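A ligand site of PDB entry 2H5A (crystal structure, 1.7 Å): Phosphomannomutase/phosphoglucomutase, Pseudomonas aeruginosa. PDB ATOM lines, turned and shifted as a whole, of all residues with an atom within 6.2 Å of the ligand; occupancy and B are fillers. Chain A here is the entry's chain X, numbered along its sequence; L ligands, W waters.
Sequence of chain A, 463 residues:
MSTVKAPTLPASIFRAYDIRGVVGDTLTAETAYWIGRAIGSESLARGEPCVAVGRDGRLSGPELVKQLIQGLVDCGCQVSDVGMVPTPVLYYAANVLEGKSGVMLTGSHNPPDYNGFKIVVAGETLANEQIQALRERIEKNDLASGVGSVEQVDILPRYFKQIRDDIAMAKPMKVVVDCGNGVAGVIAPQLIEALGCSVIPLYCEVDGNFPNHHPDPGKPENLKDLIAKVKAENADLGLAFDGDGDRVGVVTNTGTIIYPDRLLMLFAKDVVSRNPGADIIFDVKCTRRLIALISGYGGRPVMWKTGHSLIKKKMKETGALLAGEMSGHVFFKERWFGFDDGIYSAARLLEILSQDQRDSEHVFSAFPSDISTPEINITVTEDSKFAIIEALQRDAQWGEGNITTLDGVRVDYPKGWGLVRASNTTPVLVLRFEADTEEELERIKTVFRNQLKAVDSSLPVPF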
ATOM      1  N   TYR A  17      -6.911  22.219  -2.656  1.00  0.00           N
ATOM      2  CA  TYR A  17      -6.559  22.131  -4.095  1.00  0.00           C
ATOM      3  C   TYR A  17      -5.429  23.059  -4.504  1.00  0.00           C
ATOM      4  O   TYR A  17      -4.751  22.833  -5.535  1.00  0.00           O
ATOM      5  CB  TYR A  17      -7.752  22.459  -4.996  1.00  0.00           C
ATOM      6  CG  TYR A  17      -9.088  21.875  -4.600  1.00  0.00           C
ATOM      7  CD1 TYR A  17      -9.190  20.585  -4.085  1.00  0.00           C
ATOM      8  CD2 TYR A  17     -10.266  22.619  -4.771  1.00  0.00           C
ATOM      9  CE1 TYR A  17     -10.421  20.047  -3.736  1.00  0.00           C
ATOM     10  CE2 TYR A  17     -11.506  22.091  -4.421  1.00  0.00           C
ATOM     11  CZ  TYR A  17     -11.581  20.807  -3.899  1.00  0.00           C
ATOM     12  OH  TYR A  17     -12.813  20.278  -3.554  1.00  0.00           O
ATOM     13  N   ARG A  20      -5.293  30.130  -1.836  1.00  0.00           N
ATOM     14  CA  ARG A  20      -6.260  31.192  -2.214  1.00  0.00           C
ATOM     15  C   ARG A  20      -6.510  32.129  -1.044  1.00  0.00           C
ATOM     16  O   ARG A  20      -6.683  31.702   0.093  1.00  0.00           O
ATOM     17  CB  ARG A  20      -7.584  30.617  -2.738  1.00  0.00           C
ATOM     18  CG  ARG A  20      -7.917  29.196  -2.287  1.00  0.00           C
ATOM     19  CD  ARG A  20      -9.441  28.917  -2.224  1.00  0.00           C
ATOM     20  NE  ARG A  20     -10.079  29.033  -3.536  1.00  0.00           N
ATOM     21  CZ  ARG A  20     -10.025  28.119  -4.500  1.00  0.00           C
ATOM     22  NH1 ARG A  20      -9.345  26.991  -4.325  1.00  0.00           N
ATOM     23  NH2 ARG A  20     -10.671  28.325  -5.651  1.00  0.00           N
ATOM     24  N   SEP A 108      -8.969  32.672  -9.835  1.00  0.00           N
ATOM     25  CA  SEP A 108     -10.009  31.848 -10.479  1.00  0.00           C
ATOM     26  CB  SEP A 108     -10.295  30.592  -9.632  1.00  0.00           C
ATOM     27  OG  SEP A 108     -11.382  29.832 -10.141  1.00  0.00           O
ATOM     28  C   SEP A 108     -11.288  32.671 -10.793  1.00  0.00           C
ATOM     29  O   SEP A 108     -11.210  33.676 -11.506  1.00  0.00           O
ATOM     30  P   SEP A 108     -11.180  28.228 -10.079  1.00  0.00           P
ATOM     31  O1P SEP A 108     -12.511  27.539  -9.544  1.00  0.00           O
ATOM     32  O2P SEP A 108      -9.930  27.758  -9.190  1.00  0.00           O
ATOM     33  O3P SEP A 108     -10.893  27.715 -11.570  1.00  0.00           O
ATOM     34  N   HIS A 109     -12.423  32.261 -10.249  1.00  0.00           N
ATOM     35  CA  HIS A 109     -13.718  32.893 -10.573  1.00  0.00           C
ATOM     36  C   HIS A 109     -14.164  33.893  -9.508  1.00  0.00           C
ATOM     37  O   HIS A 109     -15.252  34.483  -9.604  1.00  0.00           O
ATOM     38  CB  HIS A 109     -14.788  31.810 -10.766  1.00  0.00           C
ATOM     39  CG  HIS A 109     -15.176  31.106  -9.504  1.00  0.00           C
ATOM     40  ND1 HIS A 109     -14.519  29.994  -9.032  1.00  0.00           N
ATOM     41  CD2 HIS A 109     -16.158  31.372  -8.603  1.00  0.00           C
ATOM     42  CE1 HIS A 109     -15.068  29.597  -7.904  1.00  0.00           C
ATOM     43  NE2 HIS A 109     -16.075  30.415  -7.619  1.00  0.00           N
ATOM     44  N   ARG A 247     -12.337  26.849 -16.819  1.00  0.00           N
ATOM     45  CA  ARG A 247     -13.730  26.384 -16.790  1.00  0.00           C
ATOM     46  C   ARG A 247     -14.469  26.966 -17.985  1.00  0.00           C
ATOM     47  O   ARG A 247     -14.137  28.081 -18.459  1.00  0.00           O
ATOM     48  CB  ARG A 247     -14.428  26.828 -15.502  1.00  0.00           C
ATOM     49  CG  ARG A 247     -13.810  26.241 -14.234  1.00  0.00           C
ATOM     50  CD  ARG A 247     -14.766  26.355 -13.058  1.00  0.00           C
ATOM     51  NE  ARG A 247     -15.291  27.698 -12.901  1.00  0.00           N
ATOM     52  CZ  ARG A 247     -16.254  28.024 -12.042  1.00  0.00           C
ATOM     53  NH1 ARG A 247     -16.803  27.110 -11.250  1.00  0.00           N
ATOM     54  NH2 ARG A 247     -16.670  29.283 -11.984  1.00  0.00           N
ATOM     55  N   ASP A 283     -16.670  13.796 -11.400  1.00  0.00           N
ATOM     56  CA  ASP A 283     -16.709  13.970  -9.948  1.00  0.00           C
ATOM     57  C   ASP A 283     -18.067  13.568  -9.377  1.00  0.00           C
ATOM     58  O   ASP A 283     -19.031  13.387 -10.122  1.00  0.00           O
ATOM     59  CB  ASP A 283     -16.303  15.385  -9.491  1.00  0.00           C
ATOM     60  CG  ASP A 283     -17.310  16.448  -9.859  1.00  0.00           C
ATOM     61  OD1 ASP A 283     -17.853  16.435 -10.985  1.00  0.00           O
ATOM     62  OD2 ASP A 283     -17.558  17.330  -9.016  1.00  0.00           O
ATOM     63  N   LYS A 285     -20.352  15.140  -8.147  1.00  0.00           N
ATOM     64  CA  LYS A 285     -21.438  16.081  -8.444  1.00  0.00           C
ATOM     65  C   LYS A 285     -22.159  15.842  -9.770  1.00  0.00           C
ATOM     66  O   LYS A 285     -23.191  16.479 -10.050  1.00  0.00           O
ATOM     67  CB  LYS A 285     -20.933  17.521  -8.362  1.00  0.00           C
ATOM     68  CG  LYS A 285     -20.586  17.934  -6.941  1.00  0.00           C
ATOM     69  CD  LYS A 285     -19.852  19.272  -6.879  1.00  0.00           C
ATOM     70  CE  LYS A 285     -20.763  20.449  -7.132  1.00  0.00           C
ATOM     71  NZ  LYS A 285     -19.935  21.637  -7.544  1.00  0.00           N
ATOM     72  N   THR A 306     -14.471  15.669  -5.999  1.00  0.00           N
ATOM     73  CA  THR A 306     -14.521  17.003  -6.573  1.00  0.00           C
ATOM     74  C   THR A 306     -13.186  17.718  -6.314  1.00  0.00           C
ATOM     75  O   THR A 306     -12.545  17.494  -5.253  1.00  0.00           O
ATOM     76  CB  THR A 306     -15.688  17.768  -5.914  1.00  0.00           C
ATOM     77  OG1 THR A 306     -16.928  17.133  -6.269  1.00  0.00           O
ATOM     78  CG2 THR A 306     -15.741  19.215  -6.327  1.00  0.00           C
ATOM     79  N   GLY A 307     -12.746  18.546  -7.252  1.00  0.00           N
ATOM     80  CA  GLY A 307     -11.553  19.353  -7.044  1.00  0.00           C
ATOM     81  C   GLY A 307     -10.551  19.162  -8.158  1.00  0.00           C
ATOM     82  O   GLY A 307     -10.044  18.069  -8.339  1.00  0.00           O
ATOM     83  N   HIS A 308     -10.256  20.250  -8.887  1.00  0.00           N
ATOM     84  CA  HIS A 308      -9.419  20.133 -10.092  1.00  0.00           C
ATOM     85  C   HIS A 308      -8.096  19.385  -9.841  1.00  0.00           C
ATOM     86  O   HIS A 308      -7.756  18.478 -10.612  1.00  0.00           O
ATOM     87  CB  HIS A 308      -9.193  21.512 -10.737  1.00  0.00           C
ATOM     88  CG  HIS A 308      -8.451  22.465  -9.869  1.00  0.00           C
ATOM     89  ND1 HIS A 308      -7.082  22.613  -9.915  1.00  0.00           N
ATOM     90  CD2 HIS A 308      -8.879  23.333  -8.913  1.00  0.00           C
ATOM     91  CE1 HIS A 308      -6.696  23.526  -9.044  1.00  0.00           C
ATOM     92  NE2 HIS A 308      -7.770  23.969  -8.419  1.00  0.00           N
ATOM     93  N   SER A 309      -7.388  19.707  -8.751  1.00  0.00           N
ATOM     94  CA  SER A 309      -6.095  19.076  -8.452  1.00  0.00           C
ATOM     95  C   SER A 309      -6.253  17.572  -8.189  1.00  0.00           C
ATOM     96  O   SER A 309      -5.417  16.765  -8.581  1.00  0.00           O
ATOM     97  CB  SER A 309      -5.430  19.722  -7.233  1.00  0.00           C
ATOM     98  OG  SER A 309      -5.374  21.121  -7.408  1.00  0.00           O
ATOM     99  N   GLU A 325     -15.581  17.807 -14.373  1.00  0.00           N
ATOM    100  CA  GLU A 325     -16.272  18.133 -13.131  1.00  0.00           C
ATOM    101  C   GLU A 325     -17.533  18.905 -13.443  1.00  0.00           C
ATOM    102  O   GLU A 325     -17.585  19.637 -14.448  1.00  0.00           O
ATOM    103  CB  GLU A 325     -15.414  19.041 -12.270  1.00  0.00           C
ATOM    104  CG  GLU A 325     -14.117  18.467 -11.762  1.00  0.00           C
ATOM    105  CD  GLU A 325     -13.603  19.329 -10.638  1.00  0.00           C
ATOM    106  OE1 GLU A 325     -14.067  19.143  -9.501  1.00  0.00           O
ATOM    107  OE2 GLU A 325     -12.766  20.219 -10.905  1.00  0.00           O
ATOM    108  N   MET A 326     -18.528  18.784 -12.570  1.00  0.00           N
ATOM    109  CA  MET A 326     -19.777  19.546 -12.707  1.00  0.00           C
ATOM    110  C   MET A 326     -19.517  21.064 -12.759  1.00  0.00           C
ATOM    111  O   MET A 326     -20.304  21.795 -13.369  1.00  0.00           O
ATOM    112  CB  MET A 326     -20.716  19.193 -11.549  1.00  0.00           C
ATOM    113  CG  MET A 326     -22.116  19.778 -11.674  1.00  0.00           C
ATOM    114  SD  MET A 326     -22.872  19.224 -13.213  1.00  0.00           S
ATOM    115  CE  MET A 326     -24.490  20.005 -13.105  1.00  0.00           C
ATOM    116  N   SER A 327     -18.449  21.521 -12.113  1.00  0.00           N
ATOM    117  CA  SER A 327     -18.089  22.965 -12.111  1.00  0.00           C
ATOM    118  C   SER A 327     -17.634  23.486 -13.486  1.00  0.00           C
ATOM    119  O   SER A 327     -17.592  24.706 -13.715  1.00  0.00           O
ATOM    120  CB  SER A 327     -16.986  23.232 -11.100  1.00  0.00           C
ATOM    121  OG  SER A 327     -15.807  22.538 -11.473  1.00  0.00           O
ATOM    122  N   GLY A 328     -17.263  22.589 -14.394  1.00  0.00           N
ATOM    123  CA  GLY A 328     -16.890  22.980 -15.769  1.00  0.00           C
ATOM    124  C   GLY A 328     -15.403  22.867 -16.095  1.00  0.00           C
ATOM    125  O   GLY A 328     -14.966  23.317 -17.146  1.00  0.00           O
ATOM    126  N   HIS A 329     -14.646  22.292 -15.167  1.00  0.00           N
ATOM    127  CA  HIS A 329     -13.272  21.918 -15.436  1.00  0.00           C
ATOM    128  C   HIS A 329     -13.321  20.637 -16.258  1.00  0.00           C
ATOM    129  O   HIS A 329     -13.833  19.633 -15.784  1.00  0.00           O
ATOM    130  CB  HIS A 329     -12.522  21.645 -14.137  1.00  0.00           C
ATOM    131  CG  HIS A 329     -12.252  22.873 -13.317  1.00  0.00           C
ATOM    132  ND1 HIS A 329     -11.078  23.584 -13.403  1.00  0.00           N
ATOM    133  CD2 HIS A 329     -12.995  23.475 -12.359  1.00  0.00           C
ATOM    134  CE1 HIS A 329     -11.111  24.586 -12.545  1.00  0.00           C
ATOM    135  NE2 HIS A 329     -12.263  24.556 -11.902  1.00  0.00           N
ATOM    136  N   GLU A 375     -27.721  23.612  -7.242  1.00  0.00           N
ATOM    137  CA  GLU A 375     -26.868  23.282  -6.102  1.00  0.00           C
ATOM    138  C   GLU A 375     -27.404  23.892  -4.802  1.00  0.00           C
ATOM    139  O   GLU A 375     -27.880  25.027  -4.785  1.00  0.00           O
ATOM    140  CB  GLU A 375     -25.441  23.766  -6.350  1.00  0.00           C
ATOM    141  CG  GLU A 375     -24.451  23.272  -5.322  1.00  0.00           C
ATOM    142  CD  GLU A 375     -23.023  23.504  -5.748  1.00  0.00           C
ATOM    143  OE1 GLU A 375     -22.679  23.069  -6.870  1.00  0.00           O
ATOM    144  OE2 GLU A 375     -22.252  24.116  -4.966  1.00  0.00           O
ATOM    145  N   ARG A 421     -21.513  16.789   0.621  1.00  0.00           N
ATOM    146  CA  ARG A 421     -20.065  16.846   0.826  1.00  0.00           C
ATOM    147  C   ARG A 421     -19.651  18.216   1.351  1.00  0.00           C
ATOM    148  O   ARG A 421     -20.385  19.201   1.215  1.00  0.00           O
ATOM    149  CB  ARG A 421     -19.312  16.536  -0.474  1.00  0.00           C
ATOM    150  CG  ARG A 421     -19.596  17.507  -1.625  1.00  0.00           C
ATOM    151  CD  ARG A 421     -18.695  17.274  -2.835  1.00  0.00           C
ATOM    152  NE  ARG A 421     -17.311  17.708  -2.680  1.00  0.00           N
ATOM    153  CZ  ARG A 421     -16.895  18.983  -2.753  1.00  0.00           C
ATOM    154  NH1 ARG A 421     -17.763  19.971  -2.949  1.00  0.00           N
ATOM    155  NH2 ARG A 421     -15.604  19.271  -2.633  1.00  0.00           N
ATOM    156  N   ALA A 422     -18.453  18.270   1.945  1.00  0.00           N
ATOM    157  CA  ALA A 422     -17.876  19.518   2.397  1.00  0.00           C
ATOM    158  C   ALA A 422     -17.146  20.209   1.243  1.00  0.00           C
ATOM    159  O   ALA A 422     -16.371  19.562   0.528  1.00  0.00           O
ATOM    160  CB  ALA A 422     -16.906  19.251   3.551  1.00  0.00           C
ATOM    161  N   SER A 423     -17.392  21.512   1.078  1.00  0.00           N
ATOM    162  CA  SER A 423     -16.628  22.321   0.136  1.00  0.00           C
ATOM    163  C   SER A 423     -15.197  22.447   0.658  1.00  0.00           C
ATOM    164  O   SER A 423     -14.999  22.553   1.865  1.00  0.00           O
ATOM    165  CB  SER A 423     -17.249  23.716   0.057  1.00  0.00           C
ATOM    166  OG  SER A 423     -16.442  24.592  -0.691  1.00  0.00           O
ATOM    167  N   ASN A 424     -14.215  22.448  -0.237  1.00  0.00           N
ATOM    168  CA  ASN A 424     -12.826  22.723   0.134  1.00  0.00           C
ATOM    169  C   ASN A 424     -12.393  24.146  -0.237  1.00  0.00           C
ATOM    170  O   ASN A 424     -11.202  24.445  -0.267  1.00  0.00           O
ATOM    171  CB  ASN A 424     -11.886  21.720  -0.537  1.00  0.00           C
ATOM    172  CG  ASN A 424     -12.008  20.355   0.064  1.00  0.00           C
ATOM    173  OD1 ASN A 424     -11.723  20.172   1.239  1.00  0.00           O
ATOM    174  ND2 ASN A 424     -12.461  19.391  -0.729  1.00  0.00           N
ATOM    175  N   THR A 425     -13.356  25.009  -0.544  1.00  0.00           N
ATOM    176  CA  THR A 425     -13.024  26.394  -0.925  1.00  0.00           C
ATOM    177  C   THR A 425     -13.811  27.407  -0.096  1.00  0.00           C
ATOM    178  O   THR A 425     -13.455  28.608  -0.072  1.00  0.00           O
ATOM    179  CB  THR A 425     -13.275  26.673  -2.420  1.00  0.00           C
ATOM    180  OG1 THR A 425     -14.677  26.596  -2.707  1.00  0.00           O
ATOM    181  CG2 THR A 425     -12.488  25.714  -3.302  1.00  0.00           C
ATOM    182  N   THR A 426     -14.856  26.937   0.565  1.00  0.00           N
ATOM    183  CA  THR A 426     -15.780  27.781   1.344  1.00  0.00           C
ATOM    184  C   THR A 426     -16.295  26.997   2.557  1.00  0.00           C
ATOM    185  O   THR A 426     -16.273  25.756   2.544  1.00  0.00           O
ATOM    186  CB  THR A 426     -16.998  28.220   0.478  1.00  0.00           C
ATOM    187  OG1 THR A 426     -17.681  27.048   0.025  1.00  0.00           O
ATOM    188  CG2 THR A 426     -16.548  29.047  -0.718  1.00  0.00           C
ATOM    189  N   VAL A 430     -22.186  21.130   0.580  1.00  0.00           N
ATOM    190  CA  VAL A 430     -22.724  21.149  -0.780  1.00  0.00           C
ATOM    191  C   VAL A 430     -23.619  19.929  -0.958  1.00  0.00           C
ATOM    192  O   VAL A 430     -23.225  18.807  -0.617  1.00  0.00           O
ATOM    193  CB  VAL A 430     -21.584  21.086  -1.812  1.00  0.00           C
ATOM    194  CG1 VAL A 430     -22.119  21.123  -3.234  1.00  0.00           C
ATOM    195  CG2 VAL A 430     -20.560  22.219  -1.566  1.00  0.00           C
HETATM  196  C1  LIG L   1     -15.044  23.942  -6.294  1.00  0.00           C
HETATM  197  O1  LIG L   1     -14.636  23.079  -5.232  1.00  0.00           O
HETATM  198  P1  LIG L   1     -15.532  22.884  -3.899  1.00  0.00           P
HETATM  199  O2  LIG L   1     -16.828  22.228  -4.312  1.00  0.00           O
HETATM  200  O3  LIG L   1     -15.789  24.236  -3.261  1.00  0.00           O
HETATM  201  O4  LIG L   1     -14.739  22.007  -2.968  1.00  0.00           O
HETATM  202  C2  LIG L   1     -15.654  23.159  -7.464  1.00  0.00           C
HETATM  203  O5  LIG L   1     -16.836  22.458  -7.075  1.00  0.00           O
HETATM  204  C3  LIG L   1     -14.636  22.187  -8.059  1.00  0.00           C
HETATM  205  O6  LIG L   1     -15.242  21.416  -9.098  1.00  0.00           O
HETATM  206  C4  LIG L   1     -13.427  22.998  -8.531  1.00  0.00           C
HETATM  207  O7  LIG L   1     -12.365  22.169  -9.008  1.00  0.00           O
HETATM  208  C5  LIG L   1     -12.894  23.826  -7.363  1.00  0.00           C
HETATM  209  O8  LIG L   1     -13.905  24.667  -6.771  1.00  0.00           O
HETATM  210  O   HOH W   1     -19.302  22.632  -5.027  1.00  0.00           O
HETATM  211  O   HOH W   2     -17.693  20.124  -9.511  1.00  0.00           O
HETATM  212  O   HOH W   3     -18.686  24.653  -7.410  1.00  0.00           O
HETATM  213  O   HOH W   4     -13.037  27.223  -7.017  1.00  0.00           O
HETATM  214  O   HOH W   5     -18.075  25.514  -4.005  1.00  0.00           O
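Thr 306 touches the ligand (CG2 to O5, 3.5 Å).
CA of Gly 307 touches O7 of the ligand, 3.5 Å away.
CD2 of His 329 touches O7 of the ligand (3.7 Å).
Hydrophobic or aromatic side chains within 4 Å of the ligand: Tyr 17, His 308 and His 329.
Within 4 Å of the ligand: Tyr 17, Lys 285, Thr 306, Gly 307, His 308, Glu 325, Ser 327, His 329, Arg 421, Ser 423, Asn 424 and Thr 425.
The nearest printed residue that does not touch the ligand is SEP 108 (4.2 Å).
An oxygen (O3) of the ligand sits at hydrogen-bond distance from the side-chain hydroxyl (OG1) of Thr 425 (2.7 Å).
The guanidinium group of Arg 421 is in salt-bridge range of an oxygen (O2) of the ligand, at 2.8 Å.
The side-chain hydroxyl of Ser 423 sits at hydrogen-bond distance from an oxygen (O3) of the ligand (2.7 Å).
O4 of the ligand is in hydrogen-bond range of N of Asn 424, 2.8 Å away.
The backbone NH (N) of His 308 is in hydrogen-bond range of an oxygen (O7) of the ligand (2.9 Å).
An oxygen (O5) of the ligand lies within hydrogen-bond range of the side-chain amino group (NZ) of Lys 285.
The side-chain hydroxyl (OH) of Tyr 17 is in hydrogen-bond range of an oxygen (O4) of the ligand (2.7 Å).
O6 of the ligand sits at hydrogen-bond distance from OG of Ser 327 (2.7 Å).
The side-chain carboxylate of Glu 325 is in hydrogen-bond range of an oxygen (O6) of the ligand, at 2.6 Å.
A ring nitrogen (ND1) of His 308 lies close to the side-chain hydroxyl (OG) of Ser 309.
The backbone NH of Thr 425 is in hydrogen-bond range of the side-chain hydroxyl of Ser 423 (3.1 Å).
The side-chain carboxylate of Glu 325 is in hydrogen-bond range of the backbone NH of Gly 307 (2.7 Å).
The side-chain carboxylate (OE1) of Glu 375 lies within salt-bridge range of the side-chain amino group (NZ) of Lys 285 (3.2 Å).
OH of Tyr 17 sits at hydrogen-bond distance from NH2 of Arg 421, 3.1 Å away.
O of Tyr 17 sits at hydrogen-bond distance from OG of Ser 309, 2.6 Å away.
The side-chain carboxylate (OE2) of Glu 325 sits at hydrogen-bond distance from the backbone NH (N) of His 308, at 3.2 Å.
N of Val 430 is in hydrogen-bond range of O of Arg 421 (2.7 Å).
Water W1 lies within hydrogen-bond range of O2 of the ligand (2.6 Å), NZ of Lys 285 (2.8 Å) and OE2 of Glu 375 (3.3 Å).
Water W4 lies within hydrogen-bond range of O1P of SEP 108, an oxygen (O8) of the ligand and the guanidinium group (NH2) of Arg 20.
Water W3 lies within hydrogen-bond range of an oxygen (O5) of the ligand (2.9 Å) and the side-chain amino group of Lys 285 (3.3 Å).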
